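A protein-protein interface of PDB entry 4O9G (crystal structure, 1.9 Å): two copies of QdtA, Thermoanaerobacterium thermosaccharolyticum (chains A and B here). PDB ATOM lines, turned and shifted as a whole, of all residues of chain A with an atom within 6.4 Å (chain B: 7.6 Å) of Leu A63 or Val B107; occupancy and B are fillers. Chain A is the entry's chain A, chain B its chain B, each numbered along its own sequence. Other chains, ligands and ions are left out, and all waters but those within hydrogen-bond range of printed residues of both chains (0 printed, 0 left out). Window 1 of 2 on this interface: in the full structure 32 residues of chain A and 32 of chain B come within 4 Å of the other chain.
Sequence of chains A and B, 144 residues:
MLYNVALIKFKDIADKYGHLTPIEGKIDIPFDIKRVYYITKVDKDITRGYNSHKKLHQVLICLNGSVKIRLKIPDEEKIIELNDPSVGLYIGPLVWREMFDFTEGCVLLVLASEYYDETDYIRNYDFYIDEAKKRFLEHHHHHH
Printed residues of chain B within 4 Å of Leu A63: Tyr B38, Thr B40 and Val B107. Printed residues of chain B within 4 Å of Gly A105: Asn B64 (3.6 Å). Of the printed residues of chain A, Lys B41 touches Pro A85. Val B107 touches just these residues of chain A: Leu A63 and Asn A64. The nearest printed residue of chain A that does not touch Thr B40 is Pro A85 (4.4 Å).
Tyr B38 touches Ile A61 (OH to CG2, 3.4 Å). Tyr B38 touches Leu A63. CG2 of Thr B40 touches O of Leu A63 (3.7 Å). Val B107 touches Leu A63 (CG1 to CD1, 3.7 Å). ND2 of Asn A64 touches O of Gly B105 (3.6 Å). Asn A64 touches Val B107. Lys B41 touches Pro A85 (NZ to CG, 3.8 Å). CG of Asn B64 touches O of Gly A105 (3.6 Å). Leu B63 touches Val A107 (O to CG2, 3.7 Å). CG2 of Val A107 touches CB of Asn B64, 3.7 Å away.
Of the 22 printed residues of chain B, 7 touch a printed residue of chain A. Hydrophobic or aromatic side chains of chain B within 4 Å of the printed part of chain A: Tyr B38, Leu B63 and Val B107. Of the 13 printed residues of chain A, 6 touch a printed residue of chain B. Printed residues of chain A that touch a printed residue of chain B: Ile A61, Leu A63, Asn A64, Pro A85, Gly A105 and Val A107. Among the printed residues, no Asp or Glu carboxylate lies within 4 Å of a Lys or Arg side-chain nitrogen of the other chain.
Leu A63 touches Val B107, and with the chains exchanged Val A107 touches Leu B63. Asn B64 touches its own counterpart, Asn A64. Asn A64 touches Gly B105, and with the chains exchanged Gly A105 touches Asn B64. Asn A64 touches Val B107, and with the chains exchanged Val A107 touches Asn B64. Positions printed for both chains: 61, 62, 63, 64, 65, 105, 106, 107, 108 and 109.
ND2 of Asn A64 lies close to ND2 of Asn B64 (3.2 Å). The side-chain hydroxyl of Tyr B38 is in hydrogen-bond range of the backbone carbonyl oxygen of Pro A85, 2.6 Å away.
O of Leu A109 is in hydrogen-bond range of N of Ile A61, 2.7 Å away. N of Leu A63 lies within hydrogen-bond range of O of Val A107 (2.8 Å). O of Gly A105 is in hydrogen-bond range of ND2 of Asn A64 (2.8 Å). The backbone carbonyl oxygen (O) of Asn A64 sits close to the side-chain sulfur (SG) of Cys A106 (3.7 Å). OG1 of Thr B40 sits at hydrogen-bond distance from NZ of Lys B41 (2.6 Å). The backbone carbonyl oxygen (O) of Gly B105 is in hydrogen-bond range of the side-chain amide nitrogen (ND2) of Asn B64 (3.1 Å).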
ATOM      1  N   ILE A  61     -15.157  13.265 -11.586  1.00  0.00           N
ATOM      2  CA  ILE A  61     -16.092  14.368 -11.752  1.00  0.00           C
ATOM      3  C   ILE A  61     -17.133  14.389 -10.615  1.00  0.00           C
ATOM      4  O   ILE A  61     -17.800  13.384 -10.364  1.00  0.00           O
ATOM      5  CB  ILE A  61     -16.849  14.218 -13.082  1.00  0.00           C
ATOM      6  CG1 ILE A  61     -15.877  13.808 -14.195  1.00  0.00           C
ATOM      7  CG2 ILE A  61     -17.565  15.517 -13.443  1.00  0.00           C
ATOM      8  CD1 ILE A  61     -16.461  12.854 -15.188  1.00  0.00           C
ATOM      9  N   CYS A  62     -17.267  15.531  -9.940  1.00  0.00           N
ATOM     10  CA  CYS A  62     -18.309  15.720  -8.908  1.00  0.00           C
ATOM     11  C   CYS A  62     -19.538  16.303  -9.569  1.00  0.00           C
ATOM     12  O   CYS A  62     -19.502  17.407 -10.089  1.00  0.00           O
ATOM     13  CB  CYS A  62     -17.853  16.679  -7.810  1.00  0.00           C
ATOM     14  SG  CYS A  62     -19.075  16.888  -6.474  1.00  0.00           S
ATOM     15  N   LEU A  63     -20.617  15.545  -9.564  1.00  0.00           N
ATOM     16  CA  LEU A  63     -21.786  15.886 -10.362  1.00  0.00           C
ATOM     17  C   LEU A  63     -22.847  16.596  -9.514  1.00  0.00           C
ATOM     18  O   LEU A  63     -23.804  17.150 -10.040  1.00  0.00           O
ATOM     19  CB  LEU A  63     -22.397  14.638 -10.999  1.00  0.00           C
ATOM     20  CG  LEU A  63     -21.575  13.772 -11.958  1.00  0.00           C
ATOM     21  CD1 LEU A  63     -22.503  12.732 -12.574  1.00  0.00           C
ATOM     22  CD2 LEU A  63     -20.954  14.611 -13.042  1.00  0.00           C
ATOM     23  N   ASN A  64     -22.668  16.566  -8.203  1.00  0.00           N
ATOM     24  CA  ASN A  64     -23.536  17.307  -7.296  1.00  0.00           C
ATOM     25  C   ASN A  64     -22.798  17.536  -6.017  1.00  0.00           C
ATOM     26  O   ASN A  64     -22.050  16.665  -5.562  1.00  0.00           O
ATOM     27  CB  ASN A  64     -24.807  16.528  -6.997  1.00  0.00           C
ATOM     28  CG  ASN A  64     -25.818  17.358  -6.198  1.00  0.00           C
ATOM     29  OD1 ASN A  64     -26.132  18.495  -6.559  1.00  0.00           O
ATOM     30  ND2 ASN A  64     -26.334  16.784  -5.131  1.00  0.00           N
ATOM     31  N   GLY A  65     -23.019  18.695  -5.416  1.00  0.00           N
ATOM     32  CA  GLY A  65     -22.327  19.027  -4.209  1.00  0.00           C
ATOM     33  C   GLY A  65     -20.854  19.205  -4.461  1.00  0.00           C
ATOM     34  O   GLY A  65     -20.438  19.731  -5.493  1.00  0.00           O
ATOM     35  N   ASP A  84     -18.003  21.346  -9.725  1.00  0.00           N
ATOM     36  CA  ASP A  84     -18.575  21.798 -10.989  1.00  0.00           C
ATOM     37  C   ASP A  84     -18.681  20.600 -11.952  1.00  0.00           C
ATOM     38  O   ASP A  84     -17.664  20.047 -12.357  1.00  0.00           O
ATOM     39  CB  ASP A  84     -17.632  22.849 -11.589  1.00  0.00           C
ATOM     40  CG  ASP A  84     -18.083  23.362 -12.944  1.00  0.00           C
ATOM     41  OD1 ASP A  84     -18.993  22.786 -13.579  1.00  0.00           O
ATOM     42  OD2 ASP A  84     -17.516  24.376 -13.385  1.00  0.00           O
ATOM     43  N   PRO A  85     -19.908  20.209 -12.326  1.00  0.00           N
ATOM     44  CA  PRO A  85     -20.054  19.008 -13.144  1.00  0.00           C
ATOM     45  C   PRO A  85     -19.349  19.088 -14.500  1.00  0.00           C
ATOM     46  O   PRO A  85     -19.134  18.064 -15.125  1.00  0.00           O
ATOM     47  CB  PRO A  85     -21.574  18.880 -13.295  1.00  0.00           C
ATOM     48  CG  PRO A  85     -22.109  19.506 -12.042  1.00  0.00           C
ATOM     49  CD  PRO A  85     -21.210  20.679 -11.812  1.00  0.00           C
ATOM     50  N   SER A  86     -18.979  20.294 -14.934  1.00  0.00           N
ATOM     51  CA  SER A  86     -18.373  20.514 -16.246  1.00  0.00           C
ATOM     52  C   SER A  86     -16.847  20.418 -16.208  1.00  0.00           C
ATOM     53  O   SER A  86     -16.170  20.726 -17.187  1.00  0.00           O
ATOM     54  CB  SER A  86     -18.792  21.895 -16.783  1.00  0.00           C
ATOM     55  OG  SER A  86     -18.092  22.958 -16.129  1.00  0.00           O
ATOM     56  N   GLY A 105     -25.581  14.869  -0.369  1.00  0.00           N
ATOM     57  CA  GLY A 105     -26.037  14.735  -1.750  1.00  0.00           C
ATOM     58  C   GLY A 105     -24.908  14.606  -2.763  1.00  0.00           C
ATOM     59  O   GLY A 105     -25.173  14.581  -3.957  1.00  0.00           O
ATOM     60  N   CYS A 106     -23.658  14.510  -2.296  1.00  0.00           N
ATOM     61  CA  CYS A 106     -22.505  14.481  -3.204  1.00  0.00           C
ATOM     62  C   CYS A 106     -22.502  13.255  -4.106  1.00  0.00           C
ATOM     63  O   CYS A 106     -22.738  12.132  -3.645  1.00  0.00           O
ATOM     64  CB  CYS A 106     -21.193  14.483  -2.438  1.00  0.00           C
ATOM     65  SG  CYS A 106     -19.736  14.571  -3.517  1.00  0.00           S
ATOM     66  N   VAL A 107     -22.168  13.478  -5.376  1.00  0.00           N
ATOM     67  CA  VAL A 107     -22.053  12.398  -6.360  1.00  0.00           C
ATOM     68  C   VAL A 107     -20.686  12.520  -7.013  1.00  0.00           C
ATOM     69  O   VAL A 107     -20.373  13.518  -7.632  1.00  0.00           O
ATOM     70  CB  VAL A 107     -23.135  12.481  -7.455  1.00  0.00           C
ATOM     71  CG1 VAL A 107     -22.924  11.402  -8.510  1.00  0.00           C
ATOM     72  CG2 VAL A 107     -24.535  12.353  -6.863  1.00  0.00           C
ATOM     73  N   LEU A 108     -19.870  11.499  -6.850  1.00  0.00           N
ATOM     74  CA  LEU A 108     -18.564  11.489  -7.492  1.00  0.00           C
ATOM     75  C   LEU A 108     -18.531  10.392  -8.544  1.00  0.00           C
ATOM     76  O   LEU A 108     -18.609   9.218  -8.219  1.00  0.00           O
ATOM     77  CB  LEU A 108     -17.487  11.238  -6.457  1.00  0.00           C
ATOM     78  CG  LEU A 108     -16.087  11.074  -7.000  1.00  0.00           C
ATOM     79  CD1 LEU A 108     -15.623  12.326  -7.716  1.00  0.00           C
ATOM     80  CD2 LEU A 108     -15.149  10.688  -5.889  1.00  0.00           C
ATOM     81  N   LEU A 109     -18.444  10.805  -9.798  1.00  0.00           N
ATOM     82  CA  LEU A 109     -18.348   9.892 -10.937  1.00  0.00           C
ATOM     83  C   LEU A 109     -16.905   9.764 -11.401  1.00  0.00           C
ATOM     84  O   LEU A 109     -16.181  10.753 -11.484  1.00  0.00           O
ATOM     85  CB  LEU A 109     -19.226  10.422 -12.076  1.00  0.00           C
ATOM     86  CG  LEU A 109     -19.144   9.685 -13.419  1.00  0.00           C
ATOM     87  CD1 LEU A 109     -19.771   8.328 -13.244  1.00  0.00           C
ATOM     88  CD2 LEU A 109     -19.859  10.475 -14.495  1.00  0.00           C
ATOM     89  N   TYR B  37     -23.345  11.068 -20.565  1.00  0.00           N
ATOM     90  CA  TYR B  37     -23.678  12.459 -20.332  1.00  0.00           C
ATOM     91  C   TYR B  37     -24.503  12.508 -19.091  1.00  0.00           C
ATOM     92  O   TYR B  37     -25.039  11.485 -18.644  1.00  0.00           O
ATOM     93  CB  TYR B  37     -24.395  13.079 -21.564  1.00  0.00           C
ATOM     94  CG  TYR B  37     -25.698  12.409 -21.985  1.00  0.00           C
ATOM     95  CD1 TYR B  37     -26.912  12.768 -21.405  1.00  0.00           C
ATOM     96  CD2 TYR B  37     -25.721  11.465 -22.989  1.00  0.00           C
ATOM     97  CE1 TYR B  37     -28.093  12.169 -21.786  1.00  0.00           C
ATOM     98  CE2 TYR B  37     -26.902  10.855 -23.377  1.00  0.00           C
ATOM     99  CZ  TYR B  37     -28.086  11.212 -22.775  1.00  0.00           C
ATOM    100  OH  TYR B  37     -29.264  10.621 -23.161  1.00  0.00           O
ATOM    101  N   TYR B  38     -24.590  13.687 -18.494  1.00  0.00           N
ATOM    102  CA  TYR B  38     -25.385  13.812 -17.303  1.00  0.00           C
ATOM    103  C   TYR B  38     -26.129  15.121 -17.265  1.00  0.00           C
ATOM    104  O   TYR B  38     -25.641  16.153 -17.734  1.00  0.00           O
ATOM    105  CB  TYR B  38     -24.531  13.666 -16.047  1.00  0.00           C
ATOM    106  CG  TYR B  38     -23.145  14.229 -16.149  1.00  0.00           C
ATOM    107  CD1 TYR B  38     -22.892  15.569 -15.867  1.00  0.00           C
ATOM    108  CD2 TYR B  38     -22.071  13.407 -16.495  1.00  0.00           C
ATOM    109  CE1 TYR B  38     -21.613  16.092 -15.955  1.00  0.00           C
ATOM    110  CE2 TYR B  38     -20.775  13.911 -16.591  1.00  0.00           C
ATOM    111  CZ  TYR B  38     -20.552  15.250 -16.306  1.00  0.00           C
ATOM    112  OH  TYR B  38     -19.281  15.745 -16.390  1.00  0.00           O
ATOM    113  N   ILE B  39     -27.301  15.050 -16.659  1.00  0.00           N
ATOM    114  CA  ILE B  39     -28.222  16.157 -16.631  1.00  0.00           C
ATOM    115  C   ILE B  39     -28.377  16.614 -15.192  1.00  0.00           C
ATOM    116  O   ILE B  39     -28.617  15.806 -14.311  1.00  0.00           O
ATOM    117  CB  ILE B  39     -29.591  15.779 -17.213  1.00  0.00           C
ATOM    118  CG1 ILE B  39     -29.467  15.636 -18.731  1.00  0.00           C
ATOM    119  CG2 ILE B  39     -30.615  16.876 -16.926  1.00  0.00           C
ATOM    120  CD1 ILE B  39     -30.427  14.644 -19.343  1.00  0.00           C
ATOM    121  N   THR B  40     -28.227  17.919 -14.970  1.00  0.00           N
ATOM    122  CA  THR B  40     -28.353  18.493 -13.627  1.00  0.00           C
ATOM    123  C   THR B  40     -29.051  19.847 -13.616  1.00  0.00           C
ATOM    124  O   THR B  40     -29.246  20.463 -14.654  1.00  0.00           O
ATOM    125  CB  THR B  40     -26.986  18.702 -12.952  1.00  0.00           C
ATOM    126  OG1 THR B  40     -26.184  19.600 -13.737  1.00  0.00           O
ATOM    127  CG2 THR B  40     -26.280  17.367 -12.769  1.00  0.00           C
ATOM    128  N   LYS B  41     -29.408  20.285 -12.413  1.00  0.00           N
ATOM    129  CA  LYS B  41     -29.904  21.646 -12.165  1.00  0.00           C
ATOM    130  C   LYS B  41     -31.100  21.925 -13.034  1.00  0.00           C
ATOM    131  O   LYS B  41     -31.184  22.975 -13.676  1.00  0.00           O
ATOM    132  CB  LYS B  41     -28.823  22.702 -12.406  1.00  0.00           C
ATOM    133  CG  LYS B  41     -27.721  22.720 -11.352  1.00  0.00           C
ATOM    134  CD  LYS B  41     -26.538  23.551 -11.834  1.00  0.00           C
ATOM    135  CE  LYS B  41     -25.229  22.766 -11.789  1.00  0.00           C
ATOM    136  NZ  LYS B  41     -25.022  21.842 -12.945  1.00  0.00           N
ATOM    137  N   ILE B  61     -29.690   6.487 -15.320  1.00  0.00           N
ATOM    138  CA  ILE B  61     -29.476   6.185 -13.896  1.00  0.00           C
ATOM    139  C   ILE B  61     -29.542   7.470 -13.089  1.00  0.00           C
ATOM    140  O   ILE B  61     -28.829   8.418 -13.402  1.00  0.00           O
ATOM    141  CB  ILE B  61     -28.071   5.607 -13.638  1.00  0.00           C
ATOM    142  CG1 ILE B  61     -27.707   4.545 -14.695  1.00  0.00           C
ATOM    143  CG2 ILE B  61     -28.005   5.044 -12.232  1.00  0.00           C
ATOM    144  CD1 ILE B  61     -26.222   4.454 -14.959  1.00  0.00           C
ATOM    145  N   CYS B  62     -30.388   7.498 -12.062  1.00  0.00           N
ATOM    146  CA  CYS B  62     -30.530   8.686 -11.222  1.00  0.00           C
ATOM    147  C   CYS B  62     -29.626   8.538 -10.024  1.00  0.00           C
ATOM    148  O   CYS B  62     -29.831   7.664  -9.226  1.00  0.00           O
ATOM    149  CB  CYS B  62     -31.963   8.874 -10.731  1.00  0.00           C
ATOM    150  SG  CYS B  62     -32.126  10.342  -9.664  1.00  0.00           S
ATOM    151  N   LEU B  63     -28.620   9.386  -9.922  1.00  0.00           N
ATOM    152  CA  LEU B  63     -27.539   9.191  -8.961  1.00  0.00           C
ATOM    153  C   LEU B  63     -27.781   9.983  -7.677  1.00  0.00           C
ATOM    154  O   LEU B  63     -27.132   9.777  -6.658  1.00  0.00           O
ATOM    155  CB  LEU B  63     -26.226   9.639  -9.590  1.00  0.00           C
ATOM    156  CG  LEU B  63     -25.752   8.882 -10.833  1.00  0.00           C
ATOM    157  CD1 LEU B  63     -24.339   9.296 -11.208  1.00  0.00           C
ATOM    158  CD2 LEU B  63     -25.793   7.378 -10.639  1.00  0.00           C
ATOM    159  N   ASN B  64     -28.704  10.926  -7.747  1.00  0.00           N
ATOM    160  CA  ASN B  64     -29.137  11.640  -6.564  1.00  0.00           C
ATOM    161  C   ASN B  64     -30.525  12.181  -6.824  1.00  0.00           C
ATOM    162  O   ASN B  64     -30.859  12.539  -7.956  1.00  0.00           O
ATOM    163  CB  ASN B  64     -28.190  12.783  -6.226  1.00  0.00           C
ATOM    164  CG  ASN B  64     -28.463  13.383  -4.834  1.00  0.00           C
ATOM    165  OD1 ASN B  64     -28.440  12.682  -3.825  1.00  0.00           O
ATOM    166  ND2 ASN B  64     -28.711  14.675  -4.789  1.00  0.00           N
ATOM    167  N   GLY B  65     -31.326  12.231  -5.766  1.00  0.00           N
ATOM    168  CA  GLY B  65     -32.689  12.712  -5.867  1.00  0.00           C
ATOM    169  C   GLY B  65     -33.550  11.754  -6.656  1.00  0.00           C
ATOM    170  O   GLY B  65     -33.421  10.544  -6.543  1.00  0.00           O
ATOM    171  N   SER B  66     -34.442  12.308  -7.454  1.00  0.00           N
ATOM    172  CA  SER B  66     -35.392  11.503  -8.169  1.00  0.00           C
ATOM    173  C   SER B  66     -35.827  12.230  -9.427  1.00  0.00           C
ATOM    174  O   SER B  66     -35.721  13.461  -9.527  1.00  0.00           O
ATOM    175  CB  SER B  66     -36.586  11.163  -7.268  1.00  0.00           C
ATOM    176  OG  SER B  66     -37.749  10.894  -8.023  1.00  0.00           O
ATOM    177  N   VAL B  67     -36.254  11.436 -10.406  1.00  0.00           N
ATOM    178  CA  VAL B  67     -36.739  11.922 -11.683  1.00  0.00           C
ATOM    179  C   VAL B  67     -37.662  10.863 -12.281  1.00  0.00           C
ATOM    180  O   VAL B  67     -37.446   9.667 -12.094  1.00  0.00           O
ATOM    181  CB  VAL B  67     -35.578  12.188 -12.672  1.00  0.00           C
ATOM    182  CG1 VAL B  67     -34.845  10.896 -12.992  1.00  0.00           C
ATOM    183  CG2 VAL B  67     -36.106  12.811 -13.954  1.00  0.00           C
ATOM    184  N   LEU B  82     -37.012   6.971 -11.211  1.00  0.00           N
ATOM    185  CA  LEU B  82     -35.653   6.557 -10.858  1.00  0.00           C
ATOM    186  C   LEU B  82     -35.236   7.346  -9.642  1.00  0.00           C
ATOM    187  O   LEU B  82     -35.302   8.567  -9.640  1.00  0.00           O
ATOM    188  CB  LEU B  82     -34.681   6.802 -12.023  1.00  0.00           C
ATOM    189  CG  LEU B  82     -35.076   6.169 -13.365  1.00  0.00           C
ATOM    190  CD1 LEU B  82     -34.099   6.534 -14.474  1.00  0.00           C
ATOM    191  CD2 LEU B  82     -35.198   4.654 -13.250  1.00  0.00           C
ATOM    192  N   PHE B 102     -37.835  16.442 -12.031  1.00  0.00           N
ATOM    193  CA  PHE B 102     -36.496  16.410 -11.464  1.00  0.00           C
ATOM    194  C   PHE B 102     -36.615  17.064 -10.104  1.00  0.00           C
ATOM    195  O   PHE B 102     -37.064  18.198 -10.006  1.00  0.00           O
ATOM    196  CB  PHE B 102     -35.490  17.185 -12.316  1.00  0.00           C
ATOM    197  CG  PHE B 102     -35.131  16.519 -13.622  1.00  0.00           C
ATOM    198  CD1 PHE B 102     -35.983  16.583 -14.713  1.00  0.00           C
ATOM    199  CD2 PHE B 102     -33.902  15.885 -13.775  1.00  0.00           C
ATOM    200  CE1 PHE B 102     -35.640  15.991 -15.919  1.00  0.00           C
ATOM    201  CE2 PHE B 102     -33.549  15.305 -14.977  1.00  0.00           C
ATOM    202  CZ  PHE B 102     -34.416  15.350 -16.054  1.00  0.00           C
ATOM    203  N   THR B 103     -36.208  16.352  -9.062  1.00  0.00           N
ATOM    204  CA  THR B 103     -36.040  16.963  -7.761  1.00  0.00           C
ATOM    205  C   THR B 103     -34.768  17.810  -7.772  1.00  0.00           C
ATOM    206  O   THR B 103     -34.011  17.798  -8.742  1.00  0.00           O
ATOM    207  CB  THR B 103     -36.006  15.903  -6.651  1.00  0.00           C
ATOM    208  OG1 THR B 103     -34.833  15.100  -6.774  1.00  0.00           O
ATOM    209  CG2 THR B 103     -37.238  15.017  -6.730  1.00  0.00           C
ATOM    210  N   GLU B 104     -34.542  18.583  -6.719  1.00  0.00           N
ATOM    211  CA  GLU B 104     -33.239  19.211  -6.561  1.00  0.00           C
ATOM    212  C   GLU B 104     -32.394  18.287  -5.679  1.00  0.00           C
ATOM    213  O   GLU B 104     -32.947  17.413  -5.012  1.00  0.00           O
ATOM    214  CB  GLU B 104     -33.402  20.616  -5.971  1.00  0.00           C
ATOM    215  CG  GLU B 104     -32.892  20.797  -4.553  1.00  0.00           C
ATOM    216  CD  GLU B 104     -32.732  22.257  -4.199  1.00  0.00           C
ATOM    217  OE1 GLU B 104     -32.103  22.989  -4.996  1.00  0.00           O
ATOM    218  OE2 GLU B 104     -33.243  22.670  -3.134  1.00  0.00           O
ATOM    219  N   GLY B 105     -31.069  18.403  -5.712  1.00  0.00           N
ATOM    220  CA  GLY B 105     -30.278  18.417  -6.939  1.00  0.00           C
ATOM    221  C   GLY B 105     -30.143  17.028  -7.561  1.00  0.00           C
ATOM    222  O   GLY B 105     -29.133  16.354  -7.412  1.00  0.00           O
ATOM    223  N   CYS B 106     -31.198  16.619  -8.252  1.00  0.00           N
ATOM    224  CA  CYS B 106     -31.195  15.454  -9.093  1.00  0.00           C
ATOM    225  C   CYS B 106     -30.016  15.418 -10.054  1.00  0.00           C
ATOM    226  O   CYS B 106     -29.677  16.429 -10.694  1.00  0.00           O
ATOM    227  CB  CYS B 106     -32.491  15.428  -9.890  1.00  0.00           C
ATOM    228  SG  CYS B 106     -32.708  13.961 -10.898  1.00  0.00           S
ATOM    229  N   VAL B 107     -29.402  14.238 -10.150  1.00  0.00           N
ATOM    230  CA  VAL B 107     -28.402  13.971 -11.168  1.00  0.00           C
ATOM    231  C   VAL B 107     -28.893  12.810 -12.024  1.00  0.00           C
ATOM    232  O   VAL B 107     -29.127  11.716 -11.513  1.00  0.00           O
ATOM    233  CB  VAL B 107     -27.065  13.553 -10.532  1.00  0.00           C
ATOM    234  CG1 VAL B 107     -26.027  13.231 -11.608  1.00  0.00           C
ATOM    235  CG2 VAL B 107     -26.578  14.624  -9.566  1.00  0.00           C
ATOM    236  N   LEU B 108     -29.019  13.034 -13.322  1.00  0.00           N
ATOM    237  CA  LEU B 108     -29.371  11.944 -14.222  1.00  0.00           C
ATOM    238  C   LEU B 108     -28.189  11.639 -15.117  1.00  0.00           C
ATOM    239  O   LEU B 108     -27.782  12.486 -15.906  1.00  0.00           O
ATOM    240  CB  LEU B 108     -30.573  12.326 -15.080  1.00  0.00           C
ATOM    241  CG  LEU B 108     -31.110  11.293 -16.060  1.00  0.00           C
ATOM    242  CD1 LEU B 108     -31.556  10.024 -15.353  1.00  0.00           C
ATOM    243  CD2 LEU B 108     -32.281  11.847 -16.851  1.00  0.00           C
ATOM    244  N   LEU B 109     -27.658  10.428 -14.987  1.00  0.00           N
ATOM    245  CA  LEU B 109     -26.501   9.984 -15.778  1.00  0.00           C
ATOM    246  C   LEU B 109     -26.974   9.075 -16.869  1.00  0.00           C
ATOM    247  O   LEU B 109     -27.837   8.222 -16.652  1.00  0.00           O
ATOM    248  CB  LEU B 109     -25.507   9.215 -14.893  1.00  0.00           C
ATOM    249  CG  LEU B 109     -24.355   8.494 -15.614  1.00  0.00           C
ATOM    250  CD1 LEU B 109     -23.381   9.511 -16.183  1.00  0.00           C
ATOM    251  CD2 LEU B 109     -23.658   7.570 -14.632  1.00  0.00           C
ATOM    252  N   VAL B 110     -26.396   9.240 -18.048  1.00  0.00           N
ATOM    253  CA  VAL B 110     -26.740   8.370 -19.145  1.00  0.00           C
ATOM    254  C   VAL B 110     -25.496   7.714 -19.746  1.00  0.00           C
ATOM    255  O   VAL B 110     -24.513   8.391 -20.057  1.00  0.00           O
ATOM    256  CB  VAL B 110     -27.539   9.110 -20.235  1.00  0.00           C
ATOM    257  CG1 VAL B 110     -27.911   8.155 -21.358  1.00  0.00           C
ATOM    258  CG2 VAL B 110     -28.820   9.716 -19.636  1.00  0.00           C
